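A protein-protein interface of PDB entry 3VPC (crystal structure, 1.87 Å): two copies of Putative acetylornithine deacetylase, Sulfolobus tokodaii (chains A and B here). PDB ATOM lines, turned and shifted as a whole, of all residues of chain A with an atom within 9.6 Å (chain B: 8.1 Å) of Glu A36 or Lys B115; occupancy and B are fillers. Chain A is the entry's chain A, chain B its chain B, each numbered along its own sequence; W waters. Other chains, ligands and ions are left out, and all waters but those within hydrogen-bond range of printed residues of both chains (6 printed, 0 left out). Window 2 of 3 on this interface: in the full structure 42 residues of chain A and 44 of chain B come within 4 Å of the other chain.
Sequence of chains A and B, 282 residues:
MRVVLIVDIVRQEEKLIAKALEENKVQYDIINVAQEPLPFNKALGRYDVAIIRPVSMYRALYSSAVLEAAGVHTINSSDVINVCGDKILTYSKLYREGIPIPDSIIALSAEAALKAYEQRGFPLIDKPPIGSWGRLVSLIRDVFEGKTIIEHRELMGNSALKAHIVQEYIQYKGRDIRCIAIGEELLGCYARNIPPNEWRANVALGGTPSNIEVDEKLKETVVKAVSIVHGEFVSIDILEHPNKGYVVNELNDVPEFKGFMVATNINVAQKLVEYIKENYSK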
ATOM      1  N   ILE A   6      32.584   6.566   0.013  1.00  0.00           N
ATOM      2  CA  ILE A   6      32.013   7.738  -0.677  1.00  0.00           C
ATOM      3  C   ILE A   6      32.031   7.459  -2.171  1.00  0.00           C
ATOM      4  O   ILE A   6      33.083   7.199  -2.734  1.00  0.00           O
ATOM      5  CB  ILE A   6      32.831   9.020  -0.384  1.00  0.00           C
ATOM      6  CG1 ILE A   6      32.928   9.264   1.129  1.00  0.00           C
ATOM      7  CG2 ILE A   6      32.252  10.228  -1.115  1.00  0.00           C
ATOM      8  CD1 ILE A   6      31.573   9.347   1.856  1.00  0.00           C
ATOM      9  N   VAL A   7      30.856   7.470  -2.801  1.00  0.00           N
ATOM     10  CA  VAL A   7      30.717   7.074  -4.198  1.00  0.00           C
ATOM     11  C   VAL A   7      29.880   8.131  -4.947  1.00  0.00           C
ATOM     12  O   VAL A   7      29.289   9.006  -4.323  1.00  0.00           O
ATOM     13  CB  VAL A   7      30.071   5.637  -4.331  1.00  0.00           C
ATOM     14  CG1 VAL A   7      30.839   4.615  -3.467  1.00  0.00           C
ATOM     15  CG2 VAL A   7      28.590   5.656  -3.967  1.00  0.00           C
ATOM     16  N   ASP A   8      29.889   8.076  -6.272  1.00  0.00           N
ATOM     17  CA  ASP A   8      28.855   8.749  -7.081  1.00  0.00           C
ATOM     18  C   ASP A   8      28.318   7.797  -8.159  1.00  0.00           C
ATOM     19  O   ASP A   8      27.113   7.528  -8.205  1.00  0.00           O
ATOM     20  CB  ASP A   8      29.322  10.104  -7.662  1.00  0.00           C
ATOM     21  CG  ASP A   8      30.592  10.010  -8.502  1.00  0.00           C
ATOM     22  OD1 ASP A   8      30.999  11.050  -9.066  1.00  0.00           O
ATOM     23  OD2 ASP A   8      31.212   8.935  -8.604  1.00  0.00           O
ATOM     24  N   ILE A  30      27.610   3.639   3.059  1.00  0.00           N
ATOM     25  CA  ILE A  30      27.892   4.287   1.780  1.00  0.00           C
ATOM     26  C   ILE A  30      27.175   5.636   1.796  1.00  0.00           C
ATOM     27  O   ILE A  30      26.024   5.718   2.231  1.00  0.00           O
ATOM     28  CB  ILE A  30      27.396   3.431   0.590  1.00  0.00           C
ATOM     29  CG1 ILE A  30      28.057   2.040   0.593  1.00  0.00           C
ATOM     30  CG2 ILE A  30      27.595   4.160  -0.767  1.00  0.00           C
ATOM     31  CD1 ILE A  30      27.285   0.980  -0.226  1.00  0.00           C
ATOM     32  N   ILE A  31      27.873   6.697   1.386  1.00  0.00           N
ATOM     33  CA  ILE A  31      27.209   7.947   1.059  1.00  0.00           C
ATOM     34  C   ILE A  31      27.447   8.153  -0.418  1.00  0.00           C
ATOM     35  O   ILE A  31      28.607   8.197  -0.868  1.00  0.00           O
ATOM     36  CB  ILE A  31      27.723   9.172   1.878  1.00  0.00           C
ATOM     37  CG1 ILE A  31      27.557   8.937   3.394  1.00  0.00           C
ATOM     38  CG2 ILE A  31      26.984  10.463   1.426  1.00  0.00           C
ATOM     39  CD1 ILE A  31      28.097  10.068   4.254  1.00  0.00           C
ATOM     40  N   ASN A  32      26.347   8.248  -1.167  1.00  0.00           N
ATOM     41  CA  ASN A  32      26.394   8.616  -2.574  1.00  0.00           C
ATOM     42  C   ASN A  32      26.280  10.141  -2.741  1.00  0.00           C
ATOM     43  O   ASN A  32      25.207  10.725  -2.561  1.00  0.00           O
ATOM     44  CB  ASN A  32      25.304   7.908  -3.394  1.00  0.00           C
ATOM     45  CG  ASN A  32      25.518   8.075  -4.871  1.00  0.00           C
ATOM     46  OD1 ASN A  32      25.656   9.209  -5.361  1.00  0.00           O
ATOM     47  ND2 ASN A  32      25.600   6.958  -5.597  1.00  0.00           N
ATOM     48  N   VAL A  33      27.403  10.778  -3.056  1.00  0.00           N
ATOM     49  CA  VAL A  33      27.445  12.250  -3.132  1.00  0.00           C
ATOM     50  C   VAL A  33      26.903  12.829  -4.449  1.00  0.00           C
ATOM     51  O   VAL A  33      26.849  14.052  -4.616  1.00  0.00           O
ATOM     52  CB  VAL A  33      28.858  12.799  -2.848  1.00  0.00           C
ATOM     53  CG1 VAL A  33      29.294  12.408  -1.451  1.00  0.00           C
ATOM     54  CG2 VAL A  33      29.845  12.299  -3.910  1.00  0.00           C
ATOM     55  N   ALA A  34      26.539  11.963  -5.393  1.00  0.00           N
ATOM     56  CA  ALA A  34      25.698  12.389  -6.510  1.00  0.00           C
ATOM     57  C   ALA A  34      24.221  12.492  -6.093  1.00  0.00           C
ATOM     58  O   ALA A  34      23.405  13.089  -6.818  1.00  0.00           O
ATOM     59  CB  ALA A  34      25.875  11.466  -7.742  1.00  0.00           C
ATOM     60  N   GLN A  35      23.891  11.956  -4.915  1.00  0.00           N
ATOM     61  CA  GLN A  35      22.512  11.973  -4.383  1.00  0.00           C
ATOM     62  C   GLN A  35      22.299  12.798  -3.112  1.00  0.00           C
ATOM     63  O   GLN A  35      21.221  13.364  -2.917  1.00  0.00           O
ATOM     64  CB  GLN A  35      22.030  10.549  -4.110  1.00  0.00           C
ATOM     65  CG  GLN A  35      21.887   9.675  -5.361  1.00  0.00           C
ATOM     66  CD  GLN A  35      21.761   8.205  -5.019  1.00  0.00           C
ATOM     67  OE1 GLN A  35      21.554   7.840  -3.856  1.00  0.00           O
ATOM     68  NE2 GLN A  35      21.890   7.350  -6.029  1.00  0.00           N
ATOM     69  N   GLU A  36      23.300  12.859  -2.239  1.00  0.00           N
ATOM     70  CA  GLU A  36      23.125  13.529  -0.955  1.00  0.00           C
ATOM     71  C   GLU A  36      24.045  14.737  -0.830  1.00  0.00           C
ATOM     72  O   GLU A  36      25.197  14.672  -1.281  1.00  0.00           O
ATOM     73  CB  GLU A  36      23.391  12.567   0.199  1.00  0.00           C
ATOM     74  CG  GLU A  36      22.654  11.234   0.065  1.00  0.00           C
ATOM     75  CD  GLU A  36      21.156  11.392   0.155  1.00  0.00           C
ATOM     76  OE1 GLU A  36      20.456  10.557  -0.449  1.00  0.00           O
ATOM     77  OE2 GLU A  36      20.690  12.344   0.826  1.00  0.00           O
ATOM     78  N   PRO A  37      23.542  15.836  -0.229  1.00  0.00           N
ATOM     79  CA  PRO A  37      24.449  16.934   0.064  1.00  0.00           C
ATOM     80  C   PRO A  37      25.279  16.612   1.303  1.00  0.00           C
ATOM     81  O   PRO A  37      24.937  15.704   2.073  1.00  0.00           O
ATOM     82  CB  PRO A  37      23.518  18.116   0.333  1.00  0.00           C
ATOM     83  CG  PRO A  37      22.227  17.517   0.734  1.00  0.00           C
ATOM     84  CD  PRO A  37      22.157  16.125   0.189  1.00  0.00           C
ATOM     85  N   LEU A  38      26.346  17.379   1.489  1.00  0.00           N
ATOM     86  CA  LEU A  38      27.309  17.140   2.565  1.00  0.00           C
ATOM     87  C   LEU A  38      27.384  18.349   3.481  1.00  0.00           C
ATOM     88  O   LEU A  38      27.961  19.375   3.124  1.00  0.00           O
ATOM     89  CB  LEU A  38      28.686  16.840   1.970  1.00  0.00           C
ATOM     90  CG  LEU A  38      28.854  15.521   1.221  1.00  0.00           C
ATOM     91  CD1 LEU A  38      30.131  15.533   0.396  1.00  0.00           C
ATOM     92  CD2 LEU A  38      28.869  14.369   2.220  1.00  0.00           C
ATOM     93  N   PRO A  39      26.813  18.239   4.686  1.00  0.00           N
ATOM     94  CA  PRO A  39      26.856  19.392   5.583  1.00  0.00           C
ATOM     95  C   PRO A  39      28.214  19.523   6.261  1.00  0.00           C
ATOM     96  O   PRO A  39      28.914  18.528   6.413  1.00  0.00           O
ATOM     97  CB  PRO A  39      25.805  19.037   6.625  1.00  0.00           C
ATOM     98  CG  PRO A  39      25.926  17.532   6.739  1.00  0.00           C
ATOM     99  CD  PRO A  39      26.179  17.064   5.318  1.00  0.00           C
ATOM    100  N   LEU A  44      29.475  13.569  11.181  1.00  0.00           N
ATOM    101  CA  LEU A  44      30.210  12.711  10.230  1.00  0.00           C
ATOM    102  C   LEU A  44      31.468  12.141  10.885  1.00  0.00           C
ATOM    103  O   LEU A  44      32.047  11.163  10.399  1.00  0.00           O
ATOM    104  CB  LEU A  44      30.571  13.451   8.935  1.00  0.00           C
ATOM    105  CG  LEU A  44      29.525  13.609   7.828  1.00  0.00           C
ATOM    106  CD1 LEU A  44      30.004  14.636   6.794  1.00  0.00           C
ATOM    107  CD2 LEU A  44      29.191  12.267   7.157  1.00  0.00           C
ATOM    108  N   ARG A  59      34.135  15.957  -7.195  1.00  0.00           N
ATOM    109  CA  ARG A  59      33.413  15.226  -6.150  1.00  0.00           C
ATOM    110  C   ARG A  59      34.313  14.529  -5.128  1.00  0.00           C
ATOM    111  O   ARG A  59      34.013  14.538  -3.954  1.00  0.00           O
ATOM    112  CB  ARG A  59      32.419  14.240  -6.763  1.00  0.00           C
ATOM    113  CG  ARG A  59      31.257  14.953  -7.450  1.00  0.00           C
ATOM    114  CD  ARG A  59      30.143  14.015  -7.765  1.00  0.00           C
ATOM    115  NE  ARG A  59      29.013  14.663  -8.433  1.00  0.00           N
ATOM    116  CZ  ARG A  59      28.323  14.097  -9.415  1.00  0.00           C
ATOM    117  NH1 ARG A  59      27.292  14.728  -9.987  1.00  0.00           N
ATOM    118  NH2 ARG A  59      28.686  12.901  -9.841  1.00  0.00           N
ATOM    119  N   SER A  63      34.196  16.011  -1.382  1.00  0.00           N
ATOM    120  CA  SER A  63      33.740  15.073  -0.364  1.00  0.00           C
ATOM    121  C   SER A  63      34.832  14.804   0.683  1.00  0.00           C
ATOM    122  O   SER A  63      34.560  14.828   1.886  1.00  0.00           O
ATOM    123  CB  SER A  63      33.216  13.775  -0.998  1.00  0.00           C
ATOM    124  OG  SER A  63      34.259  13.133  -1.692  1.00  0.00           O
ATOM    125  N   VAL A  66      35.034  17.983   2.990  1.00  0.00           N
ATOM    126  CA  VAL A  66      33.953  18.042   3.989  1.00  0.00           C
ATOM    127  C   VAL A  66      34.143  17.010   5.129  1.00  0.00           C
ATOM    128  O   VAL A  66      33.953  17.330   6.307  1.00  0.00           O
ATOM    129  CB  VAL A  66      32.542  17.938   3.347  1.00  0.00           C
ATOM    130  CG1 VAL A  66      31.466  17.926   4.425  1.00  0.00           C
ATOM    131  CG2 VAL A  66      32.303  19.140   2.415  1.00  0.00           C
ATOM    132  N   ILE B 105      26.185  24.269   3.263  1.00  0.00           N
ATOM    133  CA  ILE B 105      25.956  22.878   2.858  1.00  0.00           C
ATOM    134  C   ILE B 105      26.495  22.680   1.448  1.00  0.00           C
ATOM    135  O   ILE B 105      26.254  23.501   0.550  1.00  0.00           O
ATOM    136  CB  ILE B 105      24.459  22.499   2.837  1.00  0.00           C
ATOM    137  CG1 ILE B 105      23.805  22.722   4.209  1.00  0.00           C
ATOM    138  CG2 ILE B 105      24.305  21.035   2.382  1.00  0.00           C
ATOM    139  CD1 ILE B 105      22.252  22.702   4.164  1.00  0.00           C
ATOM    140  N   ILE B 106      27.221  21.588   1.255  1.00  0.00           N
ATOM    141  CA  ILE B 106      27.899  21.368  -0.006  1.00  0.00           C
ATOM    142  C   ILE B 106      27.083  20.355  -0.806  1.00  0.00           C
ATOM    143  O   ILE B 106      26.755  19.282  -0.277  1.00  0.00           O
ATOM    144  CB  ILE B 106      29.353  20.840   0.205  1.00  0.00           C
ATOM    145  CG1 ILE B 106      30.196  21.761   1.116  1.00  0.00           C
ATOM    146  CG2 ILE B 106      30.022  20.609  -1.124  1.00  0.00           C
ATOM    147  CD1 ILE B 106      30.045  23.261   0.866  1.00  0.00           C
ATOM    148  N   ALA B 107      26.751  20.702  -2.049  1.00  0.00           N
ATOM    149  CA  ALA B 107      25.960  19.833  -2.922  1.00  0.00           C
ATOM    150  C   ALA B 107      26.683  19.656  -4.240  1.00  0.00           C
ATOM    151  O   ALA B 107      27.051  20.640  -4.897  1.00  0.00           O
ATOM    152  CB  ALA B 107      24.555  20.422  -3.150  1.00  0.00           C
ATOM    153  N   LEU B 108      26.859  18.398  -4.641  1.00  0.00           N
ATOM    154  CA  LEU B 108      27.755  18.068  -5.748  1.00  0.00           C
ATOM    155  C   LEU B 108      27.033  17.548  -6.973  1.00  0.00           C
ATOM    156  O   LEU B 108      27.663  17.006  -7.871  1.00  0.00           O
ATOM    157  CB  LEU B 108      28.854  17.078  -5.296  1.00  0.00           C
ATOM    158  CG  LEU B 108      29.635  17.489  -4.042  1.00  0.00           C
ATOM    159  CD1 LEU B 108      30.567  16.342  -3.623  1.00  0.00           C
ATOM    160  CD2 LEU B 108      30.411  18.802  -4.269  1.00  0.00           C
ATOM    161  N   SER B 109      25.715  17.730  -6.994  1.00  0.00           N
ATOM    162  CA  SER B 109      24.864  17.319  -8.107  1.00  0.00           C
ATOM    163  C   SER B 109      23.559  18.092  -8.062  1.00  0.00           C
ATOM    164  O   SER B 109      23.239  18.723  -7.063  1.00  0.00           O
ATOM    165  CB  SER B 109      24.571  15.817  -8.044  1.00  0.00           C
ATOM    166  OG  SER B 109      23.653  15.564  -7.015  1.00  0.00           O
ATOM    167  N   ALA B 110      22.797  18.027  -9.154  1.00  0.00           N
ATOM    168  CA  ALA B 110      21.488  18.659  -9.216  1.00  0.00           C
ATOM    169  C   ALA B 110      20.577  18.130  -8.139  1.00  0.00           C
ATOM    170  O   ALA B 110      19.890  18.895  -7.471  1.00  0.00           O
ATOM    171  CB  ALA B 110      20.853  18.471 -10.622  1.00  0.00           C
ATOM    172  N   GLU B 111      20.602  16.817  -7.936  1.00  0.00           N
ATOM    173  CA  GLU B 111      19.727  16.201  -6.932  1.00  0.00           C
ATOM    174  C   GLU B 111      20.105  16.621  -5.517  1.00  0.00           C
ATOM    175  O   GLU B 111      19.245  17.007  -4.729  1.00  0.00           O
ATOM    176  CB  GLU B 111      19.678  14.666  -7.085  1.00  0.00           C
ATOM    177  CG  GLU B 111      18.961  13.998  -5.912  1.00  0.00           C
ATOM    178  CD  GLU B 111      19.042  12.475  -5.913  1.00  0.00           C
ATOM    179  OE1 GLU B 111      19.509  11.887  -6.901  1.00  0.00           O
ATOM    180  OE2 GLU B 111      18.652  11.878  -4.884  1.00  0.00           O
ATOM    181  N   ALA B 112      21.400  16.545  -5.189  1.00  0.00           N
ATOM    182  CA  ALA B 112      21.895  16.990  -3.881  1.00  0.00           C
ATOM    183  C   ALA B 112      21.571  18.454  -3.599  1.00  0.00           C
ATOM    184  O   ALA B 112      21.267  18.826  -2.474  1.00  0.00           O
ATOM    185  CB  ALA B 112      23.436  16.771  -3.783  1.00  0.00           C
ATOM    186  N   ALA B 113      21.693  19.284  -4.634  1.00  0.00           N
ATOM    187  CA  ALA B 113      21.467  20.714  -4.513  1.00  0.00           C
ATOM    188  C   ALA B 113      20.027  21.020  -4.116  1.00  0.00           C
ATOM    189  O   ALA B 113      19.780  21.799  -3.199  1.00  0.00           O
ATOM    190  CB  ALA B 113      21.838  21.422  -5.823  1.00  0.00           C
ATOM    191  N   LEU B 114      19.079  20.402  -4.816  1.00  0.00           N
ATOM    192  CA  LEU B 114      17.654  20.536  -4.460  1.00  0.00           C
ATOM    193  C   LEU B 114      17.358  20.127  -3.015  1.00  0.00           C
ATOM    194  O   LEU B 114      16.571  20.784  -2.338  1.00  0.00           O
ATOM    195  CB  LEU B 114      16.794  19.698  -5.404  1.00  0.00           C
ATOM    196  CG  LEU B 114      15.855  20.312  -6.428  1.00  0.00           C
ATOM    197  CD1 LEU B 114      14.654  19.381  -6.550  1.00  0.00           C
ATOM    198  CD2 LEU B 114      15.413  21.741  -6.057  1.00  0.00           C
ATOM    199  N   LYS B 115      18.005  19.057  -2.547  1.00  0.00           N
ATOM    200  CA  LYS B 115      17.879  18.600  -1.161  1.00  0.00           C
ATOM    201  C   LYS B 115      18.444  19.617  -0.183  1.00  0.00           C
ATOM    202  O   LYS B 115      17.855  19.892   0.857  1.00  0.00           O
ATOM    203  CB  LYS B 115      18.577  17.253  -0.958  1.00  0.00           C
ATOM    204  CG  LYS B 115      17.816  16.095  -1.566  1.00  0.00           C
ATOM    205  CD  LYS B 115      18.583  14.780  -1.450  1.00  0.00           C
ATOM    206  CE  LYS B 115      17.744  13.634  -2.030  1.00  0.00           C
ATOM    207  NZ  LYS B 115      18.449  12.324  -2.001  1.00  0.00           N
ATOM    208  N   ALA B 116      19.604  20.168  -0.523  1.00  0.00           N
ATOM    209  CA  ALA B 116      20.208  21.215   0.287  1.00  0.00           C
ATOM    210  C   ALA B 116      19.291  22.439   0.427  1.00  0.00           C
ATOM    211  O   ALA B 116      19.113  22.980   1.538  1.00  0.00           O
ATOM    212  CB  ALA B 116      21.563  21.599  -0.288  1.00  0.00           C
ATOM    213  N   TYR B 117      18.712  22.873  -0.693  1.00  0.00           N
ATOM    214  CA  TYR B 117      17.783  23.987  -0.666  1.00  0.00           C
ATOM    215  C   TYR B 117      16.652  23.716   0.323  1.00  0.00           C
ATOM    216  O   TYR B 117      16.320  24.562   1.148  1.00  0.00           O
ATOM    217  CB  TYR B 117      17.167  24.226  -2.040  1.00  0.00           C
ATOM    218  CG  TYR B 117      18.088  24.693  -3.140  1.00  0.00           C
ATOM    219  CD1 TYR B 117      17.717  24.518  -4.468  1.00  0.00           C
ATOM    220  CD2 TYR B 117      19.328  25.309  -2.865  1.00  0.00           C
ATOM    221  CE1 TYR B 117      18.527  24.948  -5.515  1.00  0.00           C
ATOM    222  CE2 TYR B 117      20.158  25.747  -3.913  1.00  0.00           C
ATOM    223  CZ  TYR B 117      19.745  25.563  -5.234  1.00  0.00           C
ATOM    224  OH  TYR B 117      20.522  25.973  -6.296  1.00  0.00           O
ATOM    225  N   GLU B 118      16.059  22.535   0.222  1.00  0.00           N
ATOM    226  CA  GLU B 118      14.911  22.184   1.062  1.00  0.00           C
ATOM    227  C   GLU B 118      15.344  21.960   2.506  1.00  0.00           C
ATOM    228  O   GLU B 118      14.566  22.184   3.432  1.00  0.00           O
ATOM    229  CB  GLU B 118      14.142  20.980   0.485  1.00  0.00           C
ATOM    230  CG  GLU B 118      12.608  21.207   0.467  1.00  0.00           C
ATOM    231  CD  GLU B 118      12.208  22.485  -0.270  1.00  0.00           C
ATOM    232  OE1 GLU B 118      12.391  22.539  -1.507  1.00  0.00           O
ATOM    233  OE2 GLU B 118      11.707  23.431   0.394  1.00  0.00           O
ATOM    234  N   GLN B 119      16.605  21.574   2.712  1.00  0.00           N
ATOM    235  CA  GLN B 119      17.106  21.394   4.077  1.00  0.00           C
ATOM    236  C   GLN B 119      17.239  22.721   4.775  1.00  0.00           C
ATOM    237  O   GLN B 119      16.902  22.829   5.957  1.00  0.00           O
ATOM    238  CB  GLN B 119      18.446  20.648   4.112  1.00  0.00           C
ATOM    239  CG  GLN B 119      18.330  19.137   3.942  1.00  0.00           C
ATOM    240  CD  GLN B 119      19.684  18.459   3.824  1.00  0.00           C
ATOM    241  OE1 GLN B 119      20.726  19.103   3.938  1.00  0.00           O
ATOM    242  NE2 GLN B 119      19.672  17.148   3.591  1.00  0.00           N
ATOM    243  N   ARG B 120      17.699  23.747   4.048  1.00  0.00           N
ATOM    244  CA  ARG B 120      17.930  25.013   4.723  1.00  0.00           C
ATOM    245  C   ARG B 120      16.788  26.021   4.589  1.00  0.00           C
ATOM    246  O   ARG B 120      16.628  26.854   5.473  1.00  0.00           O
ATOM    247  CB  ARG B 120      19.317  25.610   4.420  1.00  0.00           C
ATOM    248  CG  ARG B 120      19.459  26.424   3.147  1.00  0.00           C
ATOM    249  CD  ARG B 120      20.534  27.493   3.341  1.00  0.00           C
ATOM    250  NE  ARG B 120      20.100  28.498   4.314  1.00  0.00           N
ATOM    251  CZ  ARG B 120      20.514  28.567   5.579  1.00  0.00           C
ATOM    252  NH1 ARG B 120      21.406  27.707   6.044  1.00  0.00           N
ATOM    253  NH2 ARG B 120      20.045  29.518   6.379  1.00  0.00           N
ATOM    254  N   GLY B 121      15.973  25.914   3.540  1.00  0.00           N
ATOM    255  CA  GLY B 121      14.866  26.854   3.333  1.00  0.00           C
ATOM    256  C   GLY B 121      15.319  28.139   2.651  1.00  0.00           C
ATOM    257  O   GLY B 121      16.527  28.367   2.475  1.00  0.00           O
ATOM    258  N   LEU B 124      18.171  31.867   0.366  1.00  0.00           N
ATOM    259  CA  LEU B 124      19.493  31.301   0.633  1.00  0.00           C
ATOM    260  C   LEU B 124      20.469  31.830  -0.417  1.00  0.00           C
ATOM    261  O   LEU B 124      20.053  32.355  -1.446  1.00  0.00           O
ATOM    262  CB  LEU B 124      19.422  29.772   0.606  1.00  0.00           C
ATOM    263  CG  LEU B 124      19.001  29.029  -0.662  1.00  0.00           C
ATOM    264  CD1 LEU B 124      20.166  28.861  -1.659  1.00  0.00           C
ATOM    265  CD2 LEU B 124      18.437  27.653  -0.274  1.00  0.00           C
ATOM    266  N   ILE B 150      20.564  25.635 -11.003  1.00  0.00           N
ATOM    267  CA  ILE B 150      21.175  24.294 -11.097  1.00  0.00           C
ATOM    268  C   ILE B 150      21.390  23.856 -12.551  1.00  0.00           C
ATOM    269  O   ILE B 150      22.468  23.368 -12.910  1.00  0.00           O
ATOM    270  CB  ILE B 150      20.290  23.235 -10.390  1.00  0.00           C
ATOM    271  CG1 ILE B 150      20.402  23.360  -8.870  1.00  0.00           C
ATOM    272  CG2 ILE B 150      20.678  21.789 -10.820  1.00  0.00           C
ATOM    273  CD1 ILE B 150      19.260  22.663  -8.130  1.00  0.00           C
ATOM    274  N   VAL B 166      25.674  25.978  -0.591  1.00  0.00           N
ATOM    275  CA  VAL B 166      24.342  26.438  -0.221  1.00  0.00           C
ATOM    276  C   VAL B 166      24.418  26.995   1.190  1.00  0.00           C
ATOM    277  O   VAL B 166      24.627  26.244   2.171  1.00  0.00           O
ATOM    278  CB  VAL B 166      23.334  25.263  -0.326  1.00  0.00           C
ATOM    279  CG1 VAL B 166      21.891  25.715   0.015  1.00  0.00           C
ATOM    280  CG2 VAL B 166      23.412  24.619  -1.745  1.00  0.00           C
HETATM  281  O   HOH W   1      22.585  15.221   3.469  1.00  0.00           O
HETATM  282  O   HOH W   2      26.971  17.534 -10.995  1.00  0.00           O
HETATM  283  O   HOH W   3      18.594   9.065  -4.308  1.00  0.00           O
HETATM  284  O   HOH W   4      21.766  12.135  -9.172  1.00  0.00           O
HETATM  285  O   HOH W   5      26.609  16.076  -2.848  1.00  0.00           O
HETATM  286  O   HOH W   6      18.024  12.635   1.208  1.00  0.00           O
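The backbone carbonyl oxygen of Val A7 lies within hydrogen-bond range of the backbone NH of Val A33 (2.9 Å).
The backbone carbonyl oxygen (O) of Val B166 lies within hydrogen-bond range of the backbone NH (N) of Ile B105, 2.7 Å away.
The side-chain carboxylate (OD1) of Asp A8 lies within salt-bridge range of the guanidinium group (NH2) of Arg A59 (3.1 Å).
The side-chain carboxylate of Glu B111 lies within salt-bridge range of the side-chain amino group of Lys B115 (2.9 Å).
The side-chain hydroxyl (OG) of Ser B109 lies within hydrogen-bond range of the backbone NH (N) of Ala B112, at 3.1 Å.
The side-chain amide oxygen of Asn A32 lies within hydrogen-bond range of the backbone NH of Gln A35.
Val A7 touches none of the printed residues of chain B.
Ile A31 touches none of the printed residues of chain B.
Printed residues of chain B within 4 Å of Val A33: Leu B108 (3.7 Å).
Printed residues of chain B within 4 Å of Gln A35: Glu B111 (3.6 Å), Ala B112 (3.8 Å) and Lys B115 (3.1 Å).
Of chain B, only Ala B112 (3.6 Å) and Lys B115 (3.1 Å) come within 4 Å of Glu A36.
Pro A37 touches just these residues of chain B: Ile B105 (3.7 Å), Ile B106 (3.3 Å), Ala B112 (3.6 Å), Lys B115 (3.9 Å), Ala B116 (3.9 Å) and Gln B119 (3.9 Å).
Of the printed residues of chain A, Ile B105 touches Pro A37 (3.7 Å) and Leu A38 (3.99 Å).
Of the printed residues of chain A, Ser B109 touches Ala A34 (2.5 Å) and Arg A59 (3.5 Å).
Of the printed residues of chain A, Glu B111 touches Gln A35 (3.6 Å).
Ala B112 touches just these residues of chain A: Gln A35 (3.8 Å), Glu A36 (3.6 Å) and Pro A37 (3.6 Å).
Lys B115 touches just these residues of chain A: Gln A35, Glu A36 and Pro A37.
Ala B116 touches just one residue of chain A: Pro A37 (3.9 Å).
The nearest printed residue of chain A that does not touch Lys B115 is Ala A34 (7.0 Å).
The side-chain amino group (NZ) of Lys B115 is in salt-bridge range of the side-chain carboxylate (OE1) of Glu A36, at 3.1 Å.
The backbone carbonyl oxygen (O) of Ala A34 is in hydrogen-bond range of the side-chain hydroxyl (OG) of Ser B109.
The backbone carbonyl oxygen (O) of Gln A35 sits at hydrogen-bond distance from the side-chain amino group (NZ) of Lys B115 (3.1 Å).
The backbone NH (N) of Leu A38 is in hydrogen-bond range of the backbone carbonyl oxygen (O) of Ile B106, 2.6 Å away.
The backbone carbonyl oxygen (O) of Leu B108 lies within hydrogen-bond range of the guanidinium group (NE) of Arg A59, at 2.8 Å.
No position is printed for both chains.
Water W5 lies within hydrogen-bond range of the backbone carbonyl oxygen of Glu A36, the backbone carbonyl oxygen of Val A33 and the backbone NH of Leu B108.
Water W6 bridges OE2 of Glu A36 (2.7 Å) and NZ of Lys B115 (3.3 Å).
Water W1 lies within hydrogen-bond range of O of Pro A37 (2.8 Å) and NE2 of Gln B119 (3.5 Å).
Water W3 lies within hydrogen-bond range of OE2 of Glu B111 (2.9 Å) and OE1 of Gln A35 (3.2 Å).
Water W2 lies within hydrogen-bond range of the guanidinium group (NH1) of Arg A59 and the backbone carbonyl oxygen (O) of Leu B108.
Water W4 lies within hydrogen-bond range of O of Ala A34 (3.0 Å) and OE1 of Glu B111 (3.2 Å).
Among the printed residues, merely in contact across the chains: Val A33 with Leu B108, Gln A35 with Glu B111, Gln A35 with Ala B112, Glu A36 with Ala B112, Pro A37 with Ile B105, Pro A37 with Ile B106, Pro A37 with Ala B112, Pro A37 with Lys B115, Pro A37 with Ala B116, Pro A37 with Gln B119, Leu A38 with Ile B105, Arg A59 with Ser B109 and Val A66 with Ile B106.
Of the 20 printed residues of chain B, 9 touch a printed residue of chain A.
Hydrophobic or aromatic side chains of chain B that line the printed part of chain A: Ile B105, Ile B106, Leu B108 and Ala B112.
Among the printed residues, Asp or Glu carboxylates within 4 Å of a Lys or Arg side-chain nitrogen of the other chain: Glu A36 with Lys B115.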
